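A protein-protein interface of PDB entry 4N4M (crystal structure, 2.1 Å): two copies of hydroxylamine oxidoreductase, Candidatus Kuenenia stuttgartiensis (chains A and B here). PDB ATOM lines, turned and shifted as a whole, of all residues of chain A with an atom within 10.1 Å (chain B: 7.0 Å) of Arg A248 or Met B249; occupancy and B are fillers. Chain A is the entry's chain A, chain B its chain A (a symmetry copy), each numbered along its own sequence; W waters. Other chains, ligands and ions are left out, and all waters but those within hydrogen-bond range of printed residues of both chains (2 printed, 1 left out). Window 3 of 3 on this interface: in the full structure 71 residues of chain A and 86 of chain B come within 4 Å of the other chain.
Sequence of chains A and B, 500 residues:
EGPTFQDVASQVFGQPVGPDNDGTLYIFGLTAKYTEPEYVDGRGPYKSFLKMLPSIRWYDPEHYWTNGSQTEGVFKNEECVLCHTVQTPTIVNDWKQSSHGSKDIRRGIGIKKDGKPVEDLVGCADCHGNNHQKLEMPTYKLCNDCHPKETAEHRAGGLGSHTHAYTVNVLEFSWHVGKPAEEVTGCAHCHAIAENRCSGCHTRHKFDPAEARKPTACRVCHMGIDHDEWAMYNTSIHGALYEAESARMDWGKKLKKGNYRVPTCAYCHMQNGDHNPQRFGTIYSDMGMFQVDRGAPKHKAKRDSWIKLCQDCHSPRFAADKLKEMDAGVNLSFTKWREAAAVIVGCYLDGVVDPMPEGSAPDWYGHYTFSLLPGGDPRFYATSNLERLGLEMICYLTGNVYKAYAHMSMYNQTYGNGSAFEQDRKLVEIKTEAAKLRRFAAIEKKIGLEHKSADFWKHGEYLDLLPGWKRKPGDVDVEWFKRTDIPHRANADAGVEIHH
The guanidinium group (NH2) of Arg A248 lies within hydrogen-bond range of the backbone carbonyl oxygen (O) of Ser B246, 3.1 Å away. The backbone carbonyl oxygen (O) of Ala A244 lies within hydrogen-bond range of the side-chain amino group (NZ) of Lys B214 (2.7 Å). O of Met B249 sits at hydrogen-bond distance from NH2 of Arg A248, at 3.0 Å. The guanidinium group of Arg A248 sits at hydrogen-bond distance from the backbone carbonyl oxygen of Ala B247 (3.0 Å). OE2 of Glu A243 sits at hydrogen-bond distance from OH of Tyr B242, at 2.7 Å.
Among the printed residues, pairs that only touch across the chains: Ala A247 with Ala B247, Arg A248 with Lys B214, Arg A248 with Arg B248 and Arg A248 with Trp B251.
Arg A248 touches just these residues of chain B: Lys B214, Ser B246, Ala B247, Arg B248, Met B249 and Trp B251. Met B249 touches one residue of chain A. Ser B246 touches one residue of chain A. Of chain A, only Ala A247 (3.6 Å) and Arg A248 (3.0 Å) come within 4 Å of Ala B247. No residue of chain A comes within 4 Å of Asp B250. No residue of chain A comes within 4 Å of Val B262. Printed residues of chain B within 4 Å of Ala A247: Ala B247 (3.6 Å). Of the printed residues of chain A, Lys B214 touches Ala A244 and Arg A248. Of the printed residues of chain B, Glu A243 touches Tyr B242 (2.7 Å). Printed residues of chain A within 4 Å of Trp B251: Arg A248. Asp A250 touches none of the printed residues of chain B. The nearest residue of chain A that does not touch Met B249 is Ala A247 (8.1 Å). The nearest printed residue of chain B that does not touch Ala A247 is Ser B246 (5.4 Å).
Of the 18 printed residues of chain B, 7 touch a printed residue of chain A. Hydrophobic or aromatic side chains of chain A that line the printed part of chain B: Ala A244 and Ala A247. Among the printed residues, no Asp or Glu carboxylate lies within 4 Å of a Lys or Arg side-chain nitrogen of the other chain.
Ala B247 touches its own counterpart, Ala A247. Arg A248 touches Lys B214, but with the chains exchanged Lys A214 does not touch Arg B248 (10.7 Å). Arg A248 touches Ala B247, but with the chains exchanged Ala A247 does not touch Arg B248 (5.9 Å). Arg A248 touches its own counterpart, Arg B248. 15 positions are printed for both chains.
Water W2 lies within hydrogen-bond range of NH1 of Arg A248 (2.6 Å), NZ of Lys B214 (2.9 Å), OG of Ser B246 (2.9 Å) and O of Ala A244 (3.4 Å). Water W1 lies within hydrogen-bond range of the side-chain amino group of Lys B214 and the backbone carbonyl oxygen of Ala A244.
O of Ser B246 is in hydrogen-bond range of NE1 of Trp B251, 3.0 Å away. The side-chain hydroxyl (OH) of Tyr B260 lies within hydrogen-bond range of the backbone carbonyl oxygen (O) of Trp B251 (3.3 Å).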
ATOM      1  N   LYS A 214      -2.978  22.119 -21.610  1.00  0.00           N
ATOM      2  CA  LYS A 214      -4.303  21.559 -21.367  1.00  0.00           C
ATOM      3  C   LYS A 214      -4.448  20.208 -22.070  1.00  0.00           C
ATOM      4  O   LYS A 214      -3.842  19.995 -23.115  1.00  0.00           O
ATOM      5  CB  LYS A 214      -5.377  22.528 -21.864  1.00  0.00           C
ATOM      6  CG  LYS A 214      -5.334  23.877 -21.166  1.00  0.00           C
ATOM      7  CD  LYS A 214      -6.443  24.808 -21.614  1.00  0.00           C
ATOM      8  CE  LYS A 214      -6.233  26.205 -21.013  1.00  0.00           C
ATOM      9  NZ  LYS A 214      -7.439  27.053 -21.078  1.00  0.00           N
ATOM     10  N   LEU A 241     -10.855  15.967 -11.780  1.00  0.00           N
ATOM     11  CA  LEU A 241     -10.347  17.197 -11.164  1.00  0.00           C
ATOM     12  C   LEU A 241      -9.939  18.246 -12.205  1.00  0.00           C
ATOM     13  O   LEU A 241     -10.089  19.448 -11.965  1.00  0.00           O
ATOM     14  CB  LEU A 241      -9.180  16.902 -10.217  1.00  0.00           C
ATOM     15  CG  LEU A 241      -9.519  16.178  -8.910  1.00  0.00           C
ATOM     16  CD1 LEU A 241      -8.245  16.014  -8.079  1.00  0.00           C
ATOM     17  CD2 LEU A 241     -10.602  16.908  -8.107  1.00  0.00           C
ATOM     18  N   TYR A 242      -9.404  17.807 -13.346  1.00  0.00           N
ATOM     19  CA  TYR A 242      -9.118  18.730 -14.442  1.00  0.00           C
ATOM     20  C   TYR A 242     -10.404  19.436 -14.859  1.00  0.00           C
ATOM     21  O   TYR A 242     -10.435  20.654 -14.963  1.00  0.00           O
ATOM     22  CB  TYR A 242      -8.476  18.025 -15.648  1.00  0.00           C
ATOM     23  CG  TYR A 242      -8.839  18.674 -16.966  1.00  0.00           C
ATOM     24  CD1 TYR A 242      -8.308  19.907 -17.326  1.00  0.00           C
ATOM     25  CD2 TYR A 242      -9.743  18.067 -17.836  1.00  0.00           C
ATOM     26  CE1 TYR A 242      -8.658  20.522 -18.529  1.00  0.00           C
ATOM     27  CE2 TYR A 242     -10.097  18.670 -19.036  1.00  0.00           C
ATOM     28  CZ  TYR A 242      -9.549  19.896 -19.373  1.00  0.00           C
ATOM     29  OH  TYR A 242      -9.898  20.487 -20.555  1.00  0.00           O
ATOM     30  N   GLU A 243     -11.471  18.673 -15.072  1.00  0.00           N
ATOM     31  CA  GLU A 243     -12.746  19.275 -15.455  1.00  0.00           C
ATOM     32  C   GLU A 243     -13.249  20.243 -14.376  1.00  0.00           C
ATOM     33  O   GLU A 243     -13.736  21.330 -14.690  1.00  0.00           O
ATOM     34  CB  GLU A 243     -13.798  18.206 -15.756  1.00  0.00           C
ATOM     35  CG  GLU A 243     -15.134  18.798 -16.206  1.00  0.00           C
ATOM     36  CD  GLU A 243     -16.190  17.756 -16.537  1.00  0.00           C
ATOM     37  OE1 GLU A 243     -15.837  16.597 -16.851  1.00  0.00           O
ATOM     38  OE2 GLU A 243     -17.390  18.118 -16.489  1.00  0.00           O
ATOM     39  N   ALA A 244     -13.101  19.849 -13.112  1.00  0.00           N
ATOM     40  CA  ALA A 244     -13.563  20.657 -11.984  1.00  0.00           C
ATOM     41  C   ALA A 244     -12.775  21.955 -11.826  1.00  0.00           C
ATOM     42  O   ALA A 244     -13.350  22.982 -11.468  1.00  0.00           O
ATOM     43  CB  ALA A 244     -13.500  19.849 -10.689  1.00  0.00           C
ATOM     44  N   GLU A 245     -11.473  21.917 -12.097  1.00  0.00           N
ATOM     45  CA  GLU A 245     -10.601  23.051 -11.793  1.00  0.00           C
ATOM     46  C   GLU A 245     -10.153  23.858 -13.011  1.00  0.00           C
ATOM     47  O   GLU A 245      -9.597  24.941 -12.847  1.00  0.00           O
ATOM     48  CB  GLU A 245      -9.370  22.584 -10.998  1.00  0.00           C
ATOM     49  CG  GLU A 245      -9.716  22.000  -9.632  1.00  0.00           C
ATOM     50  CD  GLU A 245      -8.534  21.905  -8.683  1.00  0.00           C
ATOM     51  OE1 GLU A 245      -8.736  21.429  -7.540  1.00  0.00           O
ATOM     52  OE2 GLU A 245      -7.413  22.299  -9.062  1.00  0.00           O
ATOM     53  N   SER A 246     -10.398  23.352 -14.218  1.00  0.00           N
ATOM     54  CA  SER A 246      -9.891  23.996 -15.436  1.00  0.00           C
ATOM     55  C   SER A 246     -10.213  25.479 -15.559  1.00  0.00           C
ATOM     56  O   SER A 246      -9.372  26.259 -15.995  1.00  0.00           O
ATOM     57  CB  SER A 246     -10.419  23.304 -16.695  1.00  0.00           C
ATOM     58  OG  SER A 246      -9.858  23.928 -17.837  1.00  0.00           O
ATOM     59  N   ALA A 247     -11.436  25.857 -15.198  1.00  0.00           N
ATOM     60  CA  ALA A 247     -11.929  27.213 -15.440  1.00  0.00           C
ATOM     61  C   ALA A 247     -11.270  28.263 -14.551  1.00  0.00           C
ATOM     62  O   ALA A 247     -11.216  29.437 -14.924  1.00  0.00           O
ATOM     63  CB  ALA A 247     -13.437  27.269 -15.273  1.00  0.00           C
ATOM     64  N   ARG A 248     -10.779  27.847 -13.387  1.00  0.00           N
ATOM     65  CA  ARG A 248     -10.248  28.780 -12.401  1.00  0.00           C
ATOM     66  C   ARG A 248      -8.755  28.595 -12.090  1.00  0.00           C
ATOM     67  O   ARG A 248      -8.149  29.478 -11.496  1.00  0.00           O
ATOM     68  CB  ARG A 248     -11.095  28.719 -11.121  1.00  0.00           C
ATOM     69  CG  ARG A 248     -12.529  29.249 -11.333  1.00  0.00           C
ATOM     70  CD  ARG A 248     -13.494  28.839 -10.223  1.00  0.00           C
ATOM     71  NE  ARG A 248     -14.888  29.214 -10.520  1.00  0.00           N
ATOM     72  CZ  ARG A 248     -15.770  28.461 -11.191  1.00  0.00           C
ATOM     73  NH1 ARG A 248     -15.433  27.262 -11.669  1.00  0.00           N
ATOM     74  NH2 ARG A 248     -17.011  28.912 -11.390  1.00  0.00           N
ATOM     75  N   MET A 249      -8.155  27.480 -12.513  1.00  0.00           N
ATOM     76  CA  MET A 249      -6.721  27.252 -12.271  1.00  0.00           C
ATOM     77  C   MET A 249      -5.829  28.139 -13.153  1.00  0.00           C
ATOM     78  O   MET A 249      -6.269  28.667 -14.180  1.00  0.00           O
ATOM     79  CB  MET A 249      -6.350  25.769 -12.431  1.00  0.00           C
ATOM     80  CG  MET A 249      -6.519  25.188 -13.817  1.00  0.00           C
ATOM     81  SD  MET A 249      -6.415  23.384 -13.777  1.00  0.00           S
ATOM     82  CE  MET A 249      -4.654  23.159 -14.087  1.00  0.00           C
ATOM     83  N   ASP A 250      -4.584  28.324 -12.720  1.00  0.00           N
ATOM     84  CA  ASP A 250      -3.630  29.168 -13.434  1.00  0.00           C
ATOM     85  C   ASP A 250      -2.833  28.349 -14.457  1.00  0.00           C
ATOM     86  O   ASP A 250      -1.856  27.684 -14.108  1.00  0.00           O
ATOM     87  CB  ASP A 250      -2.676  29.868 -12.453  1.00  0.00           C
ATOM     88  CG  ASP A 250      -1.792  30.918 -13.139  1.00  0.00           C
ATOM     89  OD1 ASP A 250      -1.059  31.643 -12.433  1.00  0.00           O
ATOM     90  OD2 ASP A 250      -1.828  31.028 -14.383  1.00  0.00           O
ATOM     91  N   TRP A 251      -3.252  28.426 -15.718  1.00  0.00           N
ATOM     92  CA  TRP A 251      -2.614  27.686 -16.812  1.00  0.00           C
ATOM     93  C   TRP A 251      -1.361  28.385 -17.335  1.00  0.00           C
ATOM     94  O   TRP A 251      -0.666  27.847 -18.193  1.00  0.00           O
ATOM     95  CB  TRP A 251      -3.594  27.492 -17.974  1.00  0.00           C
ATOM     96  CG  TRP A 251      -4.704  26.532 -17.696  1.00  0.00           C
ATOM     97  CD1 TRP A 251      -6.005  26.841 -17.435  1.00  0.00           C
ATOM     98  CD2 TRP A 251      -4.616  25.101 -17.663  1.00  0.00           C
ATOM     99  NE1 TRP A 251      -6.735  25.697 -17.249  1.00  0.00           N
ATOM    100  CE2 TRP A 251      -5.910  24.613 -17.380  1.00  0.00           C
ATOM    101  CE3 TRP A 251      -3.572  24.184 -17.853  1.00  0.00           C
ATOM    102  CZ2 TRP A 251      -6.190  23.248 -17.268  1.00  0.00           C
ATOM    103  CZ3 TRP A 251      -3.851  22.820 -17.738  1.00  0.00           C
ATOM    104  CH2 TRP A 251      -5.152  22.368 -17.449  1.00  0.00           C
ATOM    105  N   GLY A 252      -1.086  29.588 -16.830  1.00  0.00           N
ATOM    106  CA  GLY A 252       0.094  30.350 -17.222  1.00  0.00           C
ATOM    107  C   GLY A 252       1.379  29.905 -16.542  1.00  0.00           C
ATOM    108  O   GLY A 252       2.454  30.371 -16.901  1.00  0.00           O
ATOM    109  N   LYS A 253       1.268  29.017 -15.555  1.00  0.00           N
ATOM    110  CA  LYS A 253       2.430  28.478 -14.850  1.00  0.00           C
ATOM    111  C   LYS A 253       3.155  27.415 -15.682  1.00  0.00           C
ATOM    112  O   LYS A 253       2.518  26.583 -16.336  1.00  0.00           O
ATOM    113  CB  LYS A 253       2.004  27.863 -13.513  1.00  0.00           C
ATOM    114  CG  LYS A 253       1.495  28.863 -12.482  1.00  0.00           C
ATOM    115  CD  LYS A 253       2.642  29.622 -11.833  1.00  0.00           C
ATOM    116  CE  LYS A 253       2.163  30.571 -10.743  1.00  0.00           C
ATOM    117  NZ  LYS A 253       3.279  31.446 -10.269  1.00  0.00           N
ATOM    118  N   ASN A 259       3.744  23.593  -9.267  1.00  0.00           N
ATOM    119  CA  ASN A 259       2.957  24.594  -9.999  1.00  0.00           C
ATOM    120  C   ASN A 259       1.519  24.167 -10.285  1.00  0.00           C
ATOM    121  O   ASN A 259       0.696  25.007 -10.652  1.00  0.00           O
ATOM    122  CB  ASN A 259       3.646  24.972 -11.324  1.00  0.00           C
ATOM    123  CG  ASN A 259       4.750  26.002 -11.143  1.00  0.00           C
ATOM    124  OD1 ASN A 259       5.017  26.450 -10.032  1.00  0.00           O
ATOM    125  ND2 ASN A 259       5.400  26.380 -12.247  1.00  0.00           N
ATOM    126  N   TYR A 260       1.220  22.876 -10.123  1.00  0.00           N
ATOM    127  CA  TYR A 260      -0.094  22.327 -10.484  1.00  0.00           C
ATOM    128  C   TYR A 260      -0.588  21.344  -9.427  1.00  0.00           C
ATOM    129  O   TYR A 260       0.186  20.557  -8.886  1.00  0.00           O
ATOM    130  CB  TYR A 260      -0.044  21.651 -11.868  1.00  0.00           C
ATOM    131  CG  TYR A 260       0.009  22.648 -13.004  1.00  0.00           C
ATOM    132  CD1 TYR A 260      -1.162  23.146 -13.568  1.00  0.00           C
ATOM    133  CD2 TYR A 260       1.220  23.125 -13.489  1.00  0.00           C
ATOM    134  CE1 TYR A 260      -1.129  24.083 -14.588  1.00  0.00           C
ATOM    135  CE2 TYR A 260       1.262  24.064 -14.518  1.00  0.00           C
ATOM    136  CZ  TYR A 260       0.084  24.540 -15.058  1.00  0.00           C
ATOM    137  OH  TYR A 260       0.110  25.475 -16.068  1.00  0.00           O
ATOM    138  N   VAL A 262      -3.524  19.492 -10.314  1.00  0.00           N
ATOM    139  CA  VAL A 262      -4.031  18.468 -11.216  1.00  0.00           C
ATOM    140  C   VAL A 262      -3.030  18.235 -12.341  1.00  0.00           C
ATOM    141  O   VAL A 262      -2.671  19.181 -13.047  1.00  0.00           O
ATOM    142  CB  VAL A 262      -5.371  18.909 -11.835  1.00  0.00           C
ATOM    143  CG1 VAL A 262      -5.924  17.829 -12.765  1.00  0.00           C
ATOM    144  CG2 VAL A 262      -6.369  19.232 -10.738  1.00  0.00           C
ATOM    145  N   LYS B 214     -19.904  19.562  -7.588  1.00  0.00           N
ATOM    146  CA  LYS B 214     -19.800  19.436  -9.038  1.00  0.00           C
ATOM    147  C   LYS B 214     -20.049  17.988  -9.466  1.00  0.00           C
ATOM    148  O   LYS B 214     -19.740  17.068  -8.717  1.00  0.00           O
ATOM    149  CB  LYS B 214     -18.416  19.890  -9.503  1.00  0.00           C
ATOM    150  CG  LYS B 214     -18.118  21.341  -9.164  1.00  0.00           C
ATOM    151  CD  LYS B 214     -16.773  21.804  -9.687  1.00  0.00           C
ATOM    152  CE  LYS B 214     -16.456  23.210  -9.156  1.00  0.00           C
ATOM    153  NZ  LYS B 214     -15.375  23.883  -9.901  1.00  0.00           N
ATOM    154  N   LEU B 241     -26.603  22.501 -19.547  1.00  0.00           N
ATOM    155  CA  LEU B 241     -26.529  23.770 -18.815  1.00  0.00           C
ATOM    156  C   LEU B 241     -25.395  23.783 -17.782  1.00  0.00           C
ATOM    157  O   LEU B 241     -24.788  24.831 -17.544  1.00  0.00           O
ATOM    158  CB  LEU B 241     -27.865  24.103 -18.146  1.00  0.00           C
ATOM    159  CG  LEU B 241     -29.019  24.502 -19.072  1.00  0.00           C
ATOM    160  CD1 LEU B 241     -30.249  24.842 -18.228  1.00  0.00           C
ATOM    161  CD2 LEU B 241     -28.649  25.672 -19.989  1.00  0.00           C
ATOM    162  N   TYR B 242     -25.122  22.639 -17.153  1.00  0.00           N
ATOM    163  CA  TYR B 242     -23.969  22.534 -16.260  1.00  0.00           C
ATOM    164  C   TYR B 242     -22.698  22.870 -17.031  1.00  0.00           C
ATOM    165  O   TYR B 242     -21.902  23.684 -16.585  1.00  0.00           O
ATOM    166  CB  TYR B 242     -23.856  21.143 -15.614  1.00  0.00           C
ATOM    167  CG  TYR B 242     -22.423  20.743 -15.337  1.00  0.00           C
ATOM    168  CD1 TYR B 242     -21.697  21.345 -14.315  1.00  0.00           C
ATOM    169  CD2 TYR B 242     -21.783  19.786 -16.123  1.00  0.00           C
ATOM    170  CE1 TYR B 242     -20.368  20.998 -14.071  1.00  0.00           C
ATOM    171  CE2 TYR B 242     -20.461  19.433 -15.887  1.00  0.00           C
ATOM    172  CZ  TYR B 242     -19.763  20.044 -14.859  1.00  0.00           C
ATOM    173  OH  TYR B 242     -18.462  19.694 -14.628  1.00  0.00           O
ATOM    174  N   ALA B 244     -22.425  24.595 -19.760  1.00  0.00           N
ATOM    175  CA  ALA B 244     -22.508  25.992 -20.187  1.00  0.00           C
ATOM    176  C   ALA B 244     -22.210  26.973 -19.055  1.00  0.00           C
ATOM    177  O   ALA B 244     -21.592  28.011 -19.291  1.00  0.00           O
ATOM    178  CB  ALA B 244     -23.883  26.286 -20.782  1.00  0.00           C
ATOM    179  N   GLU B 245     -22.633  26.648 -17.836  1.00  0.00           N
ATOM    180  CA  GLU B 245     -22.568  27.603 -16.731  1.00  0.00           C
ATOM    181  C   GLU B 245     -21.474  27.317 -15.703  1.00  0.00           C
ATOM    182  O   GLU B 245     -21.202  28.166 -14.858  1.00  0.00           O
ATOM    183  CB  GLU B 245     -23.931  27.703 -16.026  1.00  0.00           C
ATOM    184  CG  GLU B 245     -25.040  28.243 -16.923  1.00  0.00           C
ATOM    185  CD  GLU B 245     -26.268  28.723 -16.168  1.00  0.00           C
ATOM    186  OE1 GLU B 245     -27.227  29.176 -16.836  1.00  0.00           O
ATOM    187  OE2 GLU B 245     -26.284  28.653 -14.923  1.00  0.00           O
ATOM    188  N   SER B 246     -20.844  26.145 -15.773  1.00  0.00           N
ATOM    189  CA  SER B 246     -19.873  25.736 -14.751  1.00  0.00           C
ATOM    190  C   SER B 246     -18.778  26.754 -14.463  1.00  0.00           C
ATOM    191  O   SER B 246     -18.405  26.949 -13.309  1.00  0.00           O
ATOM    192  CB  SER B 246     -19.189  24.419 -15.127  1.00  0.00           C
ATOM    193  OG  SER B 246     -18.305  24.042 -14.086  1.00  0.00           O
ATOM    194  N   ALA B 247     -18.252  27.379 -15.511  1.00  0.00           N
ATOM    195  CA  ALA B 247     -17.074  28.239 -15.388  1.00  0.00           C
ATOM    196  C   ALA B 247     -17.357  29.551 -14.664  1.00  0.00           C
ATOM    197  O   ALA B 247     -16.443  30.142 -14.085  1.00  0.00           O
ATOM    198  CB  ALA B 247     -16.477  28.522 -16.755  1.00  0.00           C
ATOM    199  N   ARG B 248     -18.607  30.004 -14.700  1.00  0.00           N
ATOM    200  CA  ARG B 248     -18.967  31.309 -14.158  1.00  0.00           C
ATOM    201  C   ARG B 248     -19.955  31.259 -12.984  1.00  0.00           C
ATOM    202  O   ARG B 248     -20.113  32.254 -12.286  1.00  0.00           O
ATOM    203  CB  ARG B 248     -19.486  32.213 -15.287  1.00  0.00           C
ATOM    204  CG  ARG B 248     -18.390  32.574 -16.310  1.00  0.00           C
ATOM    205  CD  ARG B 248     -18.946  33.119 -17.623  1.00  0.00           C
ATOM    206  NE  ARG B 248     -17.900  33.306 -18.645  1.00  0.00           N
ATOM    207  CZ  ARG B 248     -17.490  32.377 -19.519  1.00  0.00           C
ATOM    208  NH1 ARG B 248     -18.020  31.153 -19.525  1.00  0.00           N
ATOM    209  NH2 ARG B 248     -16.535  32.675 -20.403  1.00  0.00           N
ATOM    210  N   MET B 249     -20.591  30.111 -12.741  1.00  0.00           N
ATOM    211  CA  MET B 249     -21.532  29.988 -11.615  1.00  0.00           C
ATOM    212  C   MET B 249     -20.818  29.952 -10.256  1.00  0.00           C
ATOM    213  O   MET B 249     -19.618  29.669 -10.171  1.00  0.00           O
ATOM    214  CB  MET B 249     -22.457  28.773 -11.783  1.00  0.00           C
ATOM    215  CG  MET B 249     -21.785  27.418 -11.763  1.00  0.00           C
ATOM    216  SD  MET B 249     -22.913  26.129 -12.340  1.00  0.00           S
ATOM    217  CE  MET B 249     -23.626  25.604 -10.771  1.00  0.00           C
ATOM    218  N   ASP B 250     -21.562  30.275  -9.200  1.00  0.00           N
ATOM    219  CA  ASP B 250     -21.015  30.316  -7.847  1.00  0.00           C
ATOM    220  C   ASP B 250     -21.160  28.956  -7.156  1.00  0.00           C
ATOM    221  O   ASP B 250     -22.223  28.628  -6.625  1.00  0.00           O
ATOM    222  CB  ASP B 250     -21.697  31.413  -7.013  1.00  0.00           C
ATOM    223  CG  ASP B 250     -21.016  31.629  -5.655  1.00  0.00           C
ATOM    224  OD1 ASP B 250     -21.399  32.575  -4.932  1.00  0.00           O
ATOM    225  OD2 ASP B 250     -20.095  30.861  -5.304  1.00  0.00           O
ATOM    226  N   TRP B 251     -20.075  28.184  -7.152  1.00  0.00           N
ATOM    227  CA  TRP B 251     -20.055  26.845  -6.553  1.00  0.00           C
ATOM    228  C   TRP B 251     -19.856  26.887  -5.040  1.00  0.00           C
ATOM    229  O   TRP B 251     -19.902  25.851  -4.382  1.00  0.00           O
ATOM    230  CB  TRP B 251     -18.943  25.995  -7.176  1.00  0.00           C
ATOM    231  CG  TRP B 251     -19.193  25.584  -8.590  1.00  0.00           C
ATOM    232  CD1 TRP B 251     -18.605  26.098  -9.706  1.00  0.00           C
ATOM    233  CD2 TRP B 251     -20.091  24.563  -9.044  1.00  0.00           C
ATOM    234  NE1 TRP B 251     -19.071  25.459 -10.824  1.00  0.00           N
ATOM    235  CE2 TRP B 251     -19.987  24.512 -10.450  1.00  0.00           C
ATOM    236  CE3 TRP B 251     -20.968  23.679  -8.398  1.00  0.00           C
ATOM    237  CZ2 TRP B 251     -20.735  23.625 -11.228  1.00  0.00           C
ATOM    238  CZ3 TRP B 251     -21.718  22.793  -9.175  1.00  0.00           C
ATOM    239  CH2 TRP B 251     -21.592  22.774 -10.577  1.00  0.00           C
ATOM    240  N   GLY B 252     -19.617  28.081  -4.496  1.00  0.00           N
ATOM    241  CA  GLY B 252     -19.437  28.264  -3.060  1.00  0.00           C
ATOM    242  C   GLY B 252     -20.734  28.296  -2.267  1.00  0.00           C
ATOM    243  O   GLY B 252     -20.701  28.297  -1.042  1.00  0.00           O
ATOM    244  N   ASN B 259     -30.401  28.494  -4.471  1.00  0.00           N
ATOM    245  CA  ASN B 259     -28.968  28.787  -4.604  1.00  0.00           C
ATOM    246  C   ASN B 259     -28.378  28.405  -5.960  1.00  0.00           C
ATOM    247  O   ASN B 259     -27.270  28.833  -6.285  1.00  0.00           O
ATOM    248  CB  ASN B 259     -28.161  28.096  -3.488  1.00  0.00           C
ATOM    249  CG  ASN B 259     -28.177  28.871  -2.180  1.00  0.00           C
ATOM    250  OD1 ASN B 259     -28.786  29.933  -2.086  1.00  0.00           O
ATOM    251  ND2 ASN B 259     -27.502  28.335  -1.160  1.00  0.00           N
ATOM    252  N   TYR B 260     -29.108  27.606  -6.742  1.00  0.00           N
ATOM    253  CA  TYR B 260     -28.595  27.074  -8.012  1.00  0.00           C
ATOM    254  C   TYR B 260     -29.662  27.127  -9.101  1.00  0.00           C
ATOM    255  O   TYR B 260     -30.835  26.861  -8.849  1.00  0.00           O
ATOM    256  CB  TYR B 260     -28.078  25.633  -7.833  1.00  0.00           C
ATOM    257  CG  TYR B 260     -26.751  25.575  -7.109  1.00  0.00           C
ATOM    258  CD1 TYR B 260     -25.552  25.650  -7.813  1.00  0.00           C
ATOM    259  CD2 TYR B 260     -26.688  25.484  -5.724  1.00  0.00           C
ATOM    260  CE1 TYR B 260     -24.331  25.629  -7.161  1.00  0.00           C
ATOM    261  CE2 TYR B 260     -25.463  25.458  -5.060  1.00  0.00           C
ATOM    262  CZ  TYR B 260     -24.291  25.534  -5.785  1.00  0.00           C
ATOM    263  OH  TYR B 260     -23.074  25.519  -5.144  1.00  0.00           O
ATOM    264  N   ARG B 261     -29.239  27.492 -10.305  1.00  0.00           N
ATOM    265  CA  ARG B 261     -30.090  27.384 -11.484  1.00  0.00           C
ATOM    266  C   ARG B 261     -30.043  25.963 -12.030  1.00  0.00           C
ATOM    267  O   ARG B 261     -31.079  25.378 -12.358  1.00  0.00           O
ATOM    268  CB  ARG B 261     -29.646  28.368 -12.579  1.00  0.00           C
ATOM    269  CG  ARG B 261     -30.316  28.085 -13.922  1.00  0.00           C
ATOM    270  CD  ARG B 261     -30.154  29.202 -14.924  1.00  0.00           C
ATOM    271  NE  ARG B 261     -31.223  29.140 -15.921  1.00  0.00           N
ATOM    272  CZ  ARG B 261     -31.064  29.040 -17.242  1.00  0.00           C
ATOM    273  NH1 ARG B 261     -29.858  28.987 -17.805  1.00  0.00           N
ATOM    274  NH2 ARG B 261     -32.145  28.993 -18.015  1.00  0.00           N
ATOM    275  N   VAL B 262     -28.826  25.430 -12.143  1.00  0.00           N
ATOM    276  CA  VAL B 262     -28.587  24.114 -12.720  1.00  0.00           C
ATOM    277  C   VAL B 262     -28.413  23.090 -11.605  1.00  0.00           C
ATOM    278  O   VAL B 262     -27.545  23.262 -10.746  1.00  0.00           O
ATOM    279  CB  VAL B 262     -27.310  24.126 -13.580  1.00  0.00           C
ATOM    280  CG1 VAL B 262     -27.064  22.754 -14.210  1.00  0.00           C
ATOM    281  CG2 VAL B 262     -27.414  25.195 -14.652  1.00  0.00           C
ATOM    282  N   PRO B 263     -29.228  22.020 -11.614  1.00  0.00           N
ATOM    283  CA  PRO B 263     -29.087  20.961 -10.623  1.00  0.00           C
ATOM    284  C   PRO B 263     -27.968  19.989 -11.000  1.00  0.00           C
ATOM    285  O   PRO B 263     -27.799  19.674 -12.174  1.00  0.00           O
ATOM    286  CB  PRO B 263     -30.438  20.253 -10.692  1.00  0.00           C
ATOM    287  CG  PRO B 263     -30.825  20.372 -12.137  1.00  0.00           C
ATOM    288  CD  PRO B 263     -30.285  21.703 -12.595  1.00  0.00           C
ATOM    289  N   THR B 264     -27.206  19.552 -10.003  1.00  0.00           N
ATOM    290  CA  THR B 264     -26.164  18.553 -10.172  1.00  0.00           C
ATOM    291  C   THR B 264     -26.548  17.313  -9.368  1.00  0.00           C
ATOM    292  O   THR B 264     -27.541  17.328  -8.643  1.00  0.00           O
ATOM    293  CB  THR B 264     -24.813  19.073  -9.653  1.00  0.00           C
ATOM    294  OG1 THR B 264     -24.903  19.301  -8.240  1.00  0.00           O
ATOM    295  CG2 THR B 264     -24.419  20.365 -10.355  1.00  0.00           C
HETATM  296  O   HOH W   1     -13.350  22.848  -8.008  1.00  0.00           O
HETATM  297  O   HOH W   2     -15.890  24.849 -12.604  1.00  0.00           O
